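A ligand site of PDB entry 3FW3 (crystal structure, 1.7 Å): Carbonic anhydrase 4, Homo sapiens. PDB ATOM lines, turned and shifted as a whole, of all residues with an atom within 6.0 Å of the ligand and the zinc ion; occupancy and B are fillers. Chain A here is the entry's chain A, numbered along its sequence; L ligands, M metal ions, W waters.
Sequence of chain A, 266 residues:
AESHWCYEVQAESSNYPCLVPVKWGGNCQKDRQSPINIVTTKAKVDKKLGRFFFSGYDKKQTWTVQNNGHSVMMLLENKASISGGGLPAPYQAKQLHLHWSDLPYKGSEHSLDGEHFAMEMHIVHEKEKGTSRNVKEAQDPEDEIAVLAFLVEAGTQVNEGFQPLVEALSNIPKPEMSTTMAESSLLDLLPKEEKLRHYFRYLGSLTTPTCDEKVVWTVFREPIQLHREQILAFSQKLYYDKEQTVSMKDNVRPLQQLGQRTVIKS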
ATOM      1  N   TRP A   5      25.568 -13.471 -36.673  1.00  0.00           N
ATOM      2  CA  TRP A   5      24.203 -13.031 -36.253  1.00  0.00           C
ATOM      3  C   TRP A   5      24.099 -11.513 -36.195  1.00  0.00           C
ATOM      4  O   TRP A   5      25.078 -10.822 -35.939  1.00  0.00           O
ATOM      5  CB  TRP A   5      23.817 -13.649 -34.878  1.00  0.00           C
ATOM      6  CG  TRP A   5      24.530 -13.106 -33.642  1.00  0.00           C
ATOM      7  CD1 TRP A   5      25.663 -13.623 -33.031  1.00  0.00           C
ATOM      8  CD2 TRP A   5      24.133 -11.989 -32.845  1.00  0.00           C
ATOM      9  NE1 TRP A   5      25.989 -12.869 -31.920  1.00  0.00           N
ATOM     10  CE2 TRP A   5      25.059 -11.859 -31.791  1.00  0.00           C
ATOM     11  CE3 TRP A   5      23.082 -11.064 -32.934  1.00  0.00           C
ATOM     12  CZ2 TRP A   5      24.970 -10.843 -30.848  1.00  0.00           C
ATOM     13  CZ3 TRP A   5      22.993 -10.069 -31.977  1.00  0.00           C
ATOM     14  CH2 TRP A   5      23.927  -9.968 -30.959  1.00  0.00           C
ATOM     15  N   ASN A  68      31.309  -3.709 -28.676  1.00  0.00           N
ATOM     16  CA  ASN A  68      31.485  -5.117 -29.118  1.00  0.00           C
ATOM     17  C   ASN A  68      30.765  -5.460 -30.399  1.00  0.00           C
ATOM     18  O   ASN A  68      30.578  -6.673 -30.754  1.00  0.00           O
ATOM     19  CB  ASN A  68      31.073  -6.099 -28.016  1.00  0.00           C
ATOM     20  CG  ASN A  68      29.601  -6.047 -27.735  1.00  0.00           C
ATOM     21  OD1 ASN A  68      28.852  -5.384 -28.445  1.00  0.00           O
ATOM     22  ND2 ASN A  68      29.168  -6.767 -26.704  1.00  0.00           N
ATOM     23  N   HIS A  70      27.595  -5.038 -30.982  1.00  0.00           N
ATOM     24  CA  HIS A  70      26.160  -5.276 -30.715  1.00  0.00           C
ATOM     25  C   HIS A  70      25.589  -4.266 -29.699  1.00  0.00           C
ATOM     26  O   HIS A  70      24.391  -4.015 -29.675  1.00  0.00           O
ATOM     27  CB  HIS A  70      25.894  -6.682 -30.185  1.00  0.00           C
ATOM     28  CG  HIS A  70      26.635  -7.768 -30.908  1.00  0.00           C
ATOM     29  ND1 HIS A  70      26.531  -7.984 -32.261  1.00  0.00           N
ATOM     30  CD2 HIS A  70      27.513  -8.704 -30.449  1.00  0.00           C
ATOM     31  CE1 HIS A  70      27.318  -8.980 -32.612  1.00  0.00           C
ATOM     32  NE2 HIS A  70      27.915  -9.443 -31.533  1.00  0.00           N
ATOM     33  N   LYS A  94      29.709  -9.164 -13.795  1.00  0.00           N
ATOM     34  CA  LYS A  94      30.576  -9.459 -14.926  1.00  0.00           C
ATOM     35  C   LYS A  94      30.638  -8.322 -15.956  1.00  0.00           C
ATOM     36  O   LYS A  94      31.722  -7.913 -16.370  1.00  0.00           O
ATOM     37  CB  LYS A  94      30.121 -10.746 -15.594  1.00  0.00           C
ATOM     38  CG  LYS A  94      30.154 -11.999 -14.670  1.00  0.00           C
ATOM     39  CD  LYS A  94      31.576 -12.368 -14.316  1.00  0.00           C
ATOM     40  CE  LYS A  94      31.683 -13.619 -13.490  1.00  0.00           C
ATOM     41  NZ  LYS A  94      33.124 -13.828 -13.124  1.00  0.00           N
ATOM     42  N   GLN A  95      29.465  -7.829 -16.392  1.00  0.00           N
ATOM     43  CA  GLN A  95      29.392  -6.744 -17.364  1.00  0.00           C
ATOM     44  C   GLN A  95      28.076  -5.986 -17.287  1.00  0.00           C
ATOM     45  O   GLN A  95      27.116  -6.467 -16.717  1.00  0.00           O
ATOM     46  CB  GLN A  95      29.575  -7.266 -18.802  1.00  0.00           C
ATOM     47  CG  GLN A  95      28.574  -8.284 -19.180  1.00  0.00           C
ATOM     48  CD  GLN A  95      28.344  -8.309 -20.645  1.00  0.00           C
ATOM     49  OE1 GLN A  95      27.603  -7.470 -21.166  1.00  0.00           O
ATOM     50  NE2 GLN A  95      29.033  -9.206 -21.329  1.00  0.00           N
ATOM     51  N   HIS A  97      25.594  -3.643 -20.031  1.00  0.00           N
ATOM     52  CA  HIS A  97      25.422  -3.169 -21.389  1.00  0.00           C
ATOM     53  C   HIS A  97      23.995  -2.645 -21.555  1.00  0.00           C
ATOM     54  O   HIS A  97      23.172  -2.774 -20.654  1.00  0.00           O
ATOM     55  CB  HIS A  97      25.762  -4.291 -22.421  1.00  0.00           C
ATOM     56  CG  HIS A  97      24.813  -5.429 -22.370  1.00  0.00           C
ATOM     57  ND1 HIS A  97      25.011  -6.539 -21.572  1.00  0.00           N
ATOM     58  CD2 HIS A  97      23.576  -5.555 -22.908  1.00  0.00           C
ATOM     59  CE1 HIS A  97      23.952  -7.334 -21.685  1.00  0.00           C
ATOM     60  NE2 HIS A  97      23.078  -6.750 -22.485  1.00  0.00           N
ATOM     61  N   LEU A  98      23.697  -2.087 -22.738  1.00  0.00           N
ATOM     62  CA  LEU A  98      22.377  -1.500 -23.005  1.00  0.00           C
ATOM     63  C   LEU A  98      21.808  -1.890 -24.347  1.00  0.00           C
ATOM     64  O   LEU A  98      22.542  -2.321 -25.244  1.00  0.00           O
ATOM     65  CB  LEU A  98      22.429   0.010 -22.944  1.00  0.00           C
ATOM     66  CG  LEU A  98      22.849   0.538 -21.567  1.00  0.00           C
ATOM     67  CD1 LEU A  98      24.345   0.807 -21.492  1.00  0.00           C
ATOM     68  CD2 LEU A  98      22.047   1.774 -21.238  1.00  0.00           C
ATOM     69  N   HIS A  99      20.494  -1.736 -24.462  1.00  0.00           N
ATOM     70  CA  HIS A  99      19.715  -1.891 -25.697  1.00  0.00           C
ATOM     71  C   HIS A  99      18.932  -0.581 -25.868  1.00  0.00           C
ATOM     72  O   HIS A  99      18.506   0.020 -24.888  1.00  0.00           O
ATOM     73  CB  HIS A  99      18.750  -3.101 -25.577  1.00  0.00           C
ATOM     74  CG  HIS A  99      19.444  -4.395 -25.252  1.00  0.00           C
ATOM     75  ND1 HIS A  99      19.886  -5.267 -26.226  1.00  0.00           N
ATOM     76  CD2 HIS A  99      19.762  -4.963 -24.063  1.00  0.00           C
ATOM     77  CE1 HIS A  99      20.492  -6.298 -25.635  1.00  0.00           C
ATOM     78  NE2 HIS A  99      20.428  -6.132 -24.330  1.00  0.00           N
ATOM     79  N   GLU A 109      13.844  -4.098 -24.389  1.00  0.00           N
ATOM     80  CA  GLU A 109      13.651  -5.511 -24.742  1.00  0.00           C
ATOM     81  C   GLU A 109      12.407  -6.057 -24.096  1.00  0.00           C
ATOM     82  O   GLU A 109      11.509  -6.606 -24.771  1.00  0.00           O
ATOM     83  CB  GLU A 109      14.907  -6.350 -24.419  1.00  0.00           C
ATOM     84  CG  GLU A 109      16.149  -5.901 -25.188  1.00  0.00           C
ATOM     85  CD  GLU A 109      17.036  -7.096 -25.556  1.00  0.00           C
ATOM     86  OE1 GLU A 109      17.576  -7.745 -24.660  1.00  0.00           O
ATOM     87  OE2 GLU A 109      17.176  -7.414 -26.742  1.00  0.00           O
ATOM     88  N   HIS A 122      21.190  -3.656 -18.819  1.00  0.00           N
ATOM     89  CA  HIS A 122      21.329  -5.018 -18.355  1.00  0.00           C
ATOM     90  C   HIS A 122      22.623  -5.139 -17.545  1.00  0.00           C
ATOM     91  O   HIS A 122      23.719  -4.927 -18.084  1.00  0.00           O
ATOM     92  CB  HIS A 122      21.374  -5.967 -19.546  1.00  0.00           C
ATOM     93  CG  HIS A 122      20.034  -6.201 -20.167  1.00  0.00           C
ATOM     94  ND1 HIS A 122      19.858  -6.903 -21.337  1.00  0.00           N
ATOM     95  CD2 HIS A 122      18.805  -5.729 -19.834  1.00  0.00           C
ATOM     96  CE1 HIS A 122      18.572  -6.934 -21.648  1.00  0.00           C
ATOM     97  NE2 HIS A 122      17.906  -6.232 -20.741  1.00  0.00           N
ATOM     98  N   VAL A 124      24.822  -7.779 -15.793  1.00  0.00           N
ATOM     99  CA  VAL A 124      24.963  -9.225 -15.911  1.00  0.00           C
ATOM    100  C   VAL A 124      25.892  -9.786 -14.818  1.00  0.00           C
ATOM    101  O   VAL A 124      27.002  -9.302 -14.649  1.00  0.00           O
ATOM    102  CB  VAL A 124      25.532  -9.616 -17.272  1.00  0.00           C
ATOM    103  CG1 VAL A 124      25.631 -11.152 -17.408  1.00  0.00           C
ATOM    104  CG2 VAL A 124      24.724  -8.982 -18.423  1.00  0.00           C
ATOM    105  N   ILE A 145      23.064 -17.346 -14.565  1.00  0.00           N
ATOM    106  CA  ILE A 145      23.244 -15.929 -14.764  1.00  0.00           C
ATOM    107  C   ILE A 145      22.042 -15.163 -14.189  1.00  0.00           C
ATOM    108  O   ILE A 145      20.883 -15.556 -14.393  1.00  0.00           O
ATOM    109  CB  ILE A 145      23.423 -15.639 -16.266  1.00  0.00           C
ATOM    110  CG1 ILE A 145      24.742 -16.267 -16.757  1.00  0.00           C
ATOM    111  CG2 ILE A 145      23.386 -14.132 -16.547  1.00  0.00           C
ATOM    112  CD1 ILE A 145      24.937 -16.239 -18.209  1.00  0.00           C
ATOM    113  N   VAL A 147      20.498 -11.454 -14.517  1.00  0.00           N
ATOM    114  CA  VAL A 147      20.526 -10.138 -15.112  1.00  0.00           C
ATOM    115  C   VAL A 147      19.567  -9.214 -14.378  1.00  0.00           C
ATOM    116  O   VAL A 147      18.369  -9.547 -14.213  1.00  0.00           O
ATOM    117  CB  VAL A 147      20.150 -10.172 -16.658  1.00  0.00           C
ATOM    118  CG1 VAL A 147      20.220  -8.746 -17.249  1.00  0.00           C
ATOM    119  CG2 VAL A 147      21.076 -11.085 -17.428  1.00  0.00           C
ATOM    120  N   SER A 205      16.109 -16.618 -20.788  1.00  0.00           N
ATOM    121  CA  SER A 205      17.300 -16.798 -21.603  1.00  0.00           C
ATOM    122  C   SER A 205      18.138 -15.557 -21.797  1.00  0.00           C
ATOM    123  O   SER A 205      17.713 -14.437 -21.510  1.00  0.00           O
ATOM    124  CB  SER A 205      16.880 -17.336 -22.980  1.00  0.00           C
ATOM    125  OG  SER A 205      16.416 -16.277 -23.857  1.00  0.00           O
ATOM    126  N   LEU A 206      19.322 -15.764 -22.358  1.00  0.00           N
ATOM    127  CA  LEU A 206      20.080 -14.683 -22.932  1.00  0.00           C
ATOM    128  C   LEU A 206      19.288 -14.148 -24.128  1.00  0.00           C
ATOM    129  O   LEU A 206      18.590 -14.936 -24.818  1.00  0.00           O
ATOM    130  CB  LEU A 206      21.419 -15.161 -23.426  1.00  0.00           C
ATOM    131  CG  LEU A 206      22.364 -15.731 -22.375  1.00  0.00           C
ATOM    132  CD1 LEU A 206      23.610 -16.223 -23.098  1.00  0.00           C
ATOM    133  CD2 LEU A 206      22.726 -14.694 -21.348  1.00  0.00           C
ATOM    134  N   THR A 207      19.313 -12.852 -24.349  1.00  0.00           N
ATOM    135  CA  THR A 207      18.576 -12.218 -25.499  1.00  0.00           C
ATOM    136  C   THR A 207      19.395 -12.098 -26.811  1.00  0.00           C
ATOM    137  O   THR A 207      18.984 -11.407 -27.731  1.00  0.00           O
ATOM    138  CB  THR A 207      17.977 -10.851 -25.140  1.00  0.00           C
ATOM    139  OG1 THR A 207      19.033  -9.918 -24.925  1.00  0.00           O
ATOM    140  CG2 THR A 207      17.173 -10.939 -23.868  1.00  0.00           C
ATOM    141  N   THR A 208      20.560 -12.709 -26.838  1.00  0.00           N
ATOM    142  CA  THR A 208      21.386 -12.821 -28.065  1.00  0.00           C
ATOM    143  C   THR A 208      21.803 -14.275 -28.211  1.00  0.00           C
ATOM    144  O   THR A 208      21.782 -15.010 -27.240  1.00  0.00           O
ATOM    145  CB  THR A 208      22.666 -11.943 -28.008  1.00  0.00           C
ATOM    146  OG1 THR A 208      23.547 -12.414 -26.964  1.00  0.00           O
ATOM    147  CG2 THR A 208      22.392 -10.515 -27.625  1.00  0.00           C
ATOM    148  N   PRO A 209      22.206 -14.712 -29.415  1.00  0.00           N
ATOM    149  CA  PRO A 209      22.778 -16.044 -29.568  1.00  0.00           C
ATOM    150  C   PRO A 209      23.926 -16.212 -28.552  1.00  0.00           C
ATOM    151  O   PRO A 209      24.606 -15.242 -28.310  1.00  0.00           O
ATOM    152  CB  PRO A 209      23.297 -16.023 -31.012  1.00  0.00           C
ATOM    153  CG  PRO A 209      22.312 -15.163 -31.688  1.00  0.00           C
ATOM    154  CD  PRO A 209      22.123 -14.019 -30.715  1.00  0.00           C
ATOM    155  N   LYS A 214      19.407 -20.036 -19.183  1.00  0.00           N
ATOM    156  CA  LYS A 214      20.180 -20.103 -17.918  1.00  0.00           C
ATOM    157  C   LYS A 214      20.179 -18.792 -17.135  1.00  0.00           C
ATOM    158  O   LYS A 214      20.988 -18.589 -16.230  1.00  0.00           O
ATOM    159  CB  LYS A 214      21.619 -20.546 -18.175  1.00  0.00           C
ATOM    160  CG  LYS A 214      22.427 -19.568 -19.005  1.00  0.00           C
ATOM    161  CD  LYS A 214      23.732 -20.246 -19.497  1.00  0.00           C
ATOM    162  CE  LYS A 214      24.643 -19.251 -20.219  1.00  0.00           C
ATOM    163  NZ  LYS A 214      26.019 -19.784 -20.486  1.00  0.00           N
ATOM    164  N   VAL A 215      19.197 -17.942 -17.429  1.00  0.00           N
ATOM    165  CA  VAL A 215      19.123 -16.627 -16.838  1.00  0.00           C
ATOM    166  C   VAL A 215      17.929 -16.520 -15.869  1.00  0.00           C
ATOM    167  O   VAL A 215      16.780 -16.830 -16.205  1.00  0.00           O
ATOM    168  CB  VAL A 215      19.003 -15.500 -17.902  1.00  0.00           C
ATOM    169  CG1 VAL A 215      18.947 -14.128 -17.203  1.00  0.00           C
ATOM    170  CG2 VAL A 215      20.140 -15.577 -18.885  1.00  0.00           C
ATOM    171  N   TRP A 217      15.887 -13.659 -14.526  1.00  0.00           N
ATOM    172  CA  TRP A 217      15.631 -12.253 -14.823  1.00  0.00           C
ATOM    173  C   TRP A 217      14.980 -11.476 -13.695  1.00  0.00           C
ATOM    174  O   TRP A 217      14.151 -11.991 -12.987  1.00  0.00           O
ATOM    175  CB  TRP A 217      14.722 -12.128 -16.068  1.00  0.00           C
ATOM    176  CG  TRP A 217      15.486 -12.320 -17.333  1.00  0.00           C
ATOM    177  CD1 TRP A 217      15.625 -13.481 -18.024  1.00  0.00           C
ATOM    178  CD2 TRP A 217      16.283 -11.355 -18.030  1.00  0.00           C
ATOM    179  NE1 TRP A 217      16.417 -13.307 -19.117  1.00  0.00           N
ATOM    180  CE2 TRP A 217      16.821 -12.012 -19.186  1.00  0.00           C
ATOM    181  CE3 TRP A 217      16.560  -9.997 -17.853  1.00  0.00           C
ATOM    182  CZ2 TRP A 217      17.683 -11.373 -20.088  1.00  0.00           C
ATOM    183  CZ3 TRP A 217      17.330  -9.348 -18.778  1.00  0.00           C
ATOM    184  CH2 TRP A 217      17.916 -10.046 -19.884  1.00  0.00           C
HETATM  185  S1  LIG L   1      24.169 -11.277 -21.165  1.00  0.00           S
HETATM  186  C1  LIG L   1      23.100 -10.940 -22.529  1.00  0.00           C
HETATM  187  C2  LIG L   1      23.776 -11.346 -23.647  1.00  0.00           C
HETATM  188  C3  LIG L   1      25.048 -11.922 -23.444  1.00  0.00           C
HETATM  189  C4  LIG L   1      25.909 -12.538 -24.548  1.00  0.00           C
HETATM  190  C5  LIG L   1      26.899 -13.575 -23.989  1.00  0.00           C
HETATM  191  C6  LIG L   1      27.835 -13.016 -22.895  1.00  0.00           C
HETATM  192  S2  LIG L   1      26.859 -12.731 -21.414  1.00  0.00           S
HETATM  193  C7  LIG L   1      25.438 -12.013 -22.134  1.00  0.00           C
HETATM  194  S3  LIG L   1      21.536 -10.311 -22.151  1.00  0.00           S
HETATM  195  O1  LIG L   1      21.732  -9.570 -20.931  1.00  0.00           O
HETATM  196  O2  LIG L   1      20.654 -11.436 -22.204  1.00  0.00           O
HETATM  197  N1  LIG L   1      21.140  -9.351 -23.425  1.00  0.00           N
HETATM  198  N2  LIG L   1      26.663 -11.475 -25.229  1.00  0.00           N
HETATM  199  C8  LIG L   1      28.927 -14.019 -22.489  1.00  0.00           C
HETATM  200  O3  LIG L   1      26.367 -13.957 -20.942  1.00  0.00           O
HETATM  201  O4  LIG L   1      27.381 -11.750 -20.540  1.00  0.00           O
HETATM  202  C9  LIG L   1      25.910 -10.872 -26.323  1.00  0.00           C
HETATM  203  C10 LIG L   1      26.846  -9.994 -27.153  1.00  0.00           C
HETATM  204 ZN    ZN M   1      21.175  -7.394 -22.857  1.00  0.00          ZN
HETATM  205  O   HOH W   1      25.122  -7.737 -25.159  1.00  0.00           O
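An oxygen (O4) of the ligand lies within hydrogen-bond range of the side-chain amide nitrogen (NE2) of Gln 95 (3.1 Å). O2 of the ligand sits at hydrogen-bond distance from N of Thr 207 (2.9 Å). The side-chain hydroxyl (OG1) of Thr 207 sits close to a nitrogen (N1) of the ligand, at 2.6 Å.
His 70 touches the ligand (CD2 to C10, 3.6 Å). Val 124 touches the ligand (CG2 to S1, 3.6 Å). CD1 of Ile 145 touches O3 of the ligand, 3.8 Å away. Val 147 touches the ligand (CG2 to O1, 3.9 Å). CA of Leu 206 touches O2 of the ligand, 3.4 Å away. OG1 of Thr 208 touches C9 of the ligand, at 2.9 Å. Trp 217 touches the ligand. Of the 21 residues printed, 12 come within 4 Å of the ligand.
Thr 207 touches the zinc ion. Of the 21 residues printed, 4 come within 4 Å of the zinc ion.
The side-chain amide oxygen (OD1) of Asn 68 is in hydrogen-bond range of the backbone NH (N) of His 70 (2.9 Å). The backbone NH (N) of Ile 145 is in hydrogen-bond range of the backbone carbonyl oxygen (O) of Lys 214 (2.9 Å). The side-chain carboxylate (OE2) of Glu 109 lies close to a ring nitrogen (ND1) of His 99, 3.5 Å away. The backbone carbonyl oxygen (O) of Val 124 sits at hydrogen-bond distance from the backbone NH (N) of Lys 94, 2.8 Å away. The side-chain carboxylate (OE1) of Glu 109 sits at hydrogen-bond distance from the side-chain hydroxyl (OG1) of Thr 207 (2.6 Å). The backbone carbonyl oxygen of Ser 205 sits at hydrogen-bond distance from the indole nitrogen of Trp 217, at 2.9 Å. The side-chain amide oxygen (OE1) of Gln 95 lies within hydrogen-bond range of a ring nitrogen (ND1) of His 97, at 2.8 Å. O of Gln 95 sits at hydrogen-bond distance from N of Val 124, at 2.8 Å.
N1 of the ligand binds the zinc ion (2.0 Å). The zinc ion is bound by NE2 of His 97, at 2.0 Å. ND1 of His 122 binds the zinc ion, at 2.1 Å. The zinc ion is bound by NE2 of His 99, 2.1 Å away. The zinc ion has four donor atoms within binding distance.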
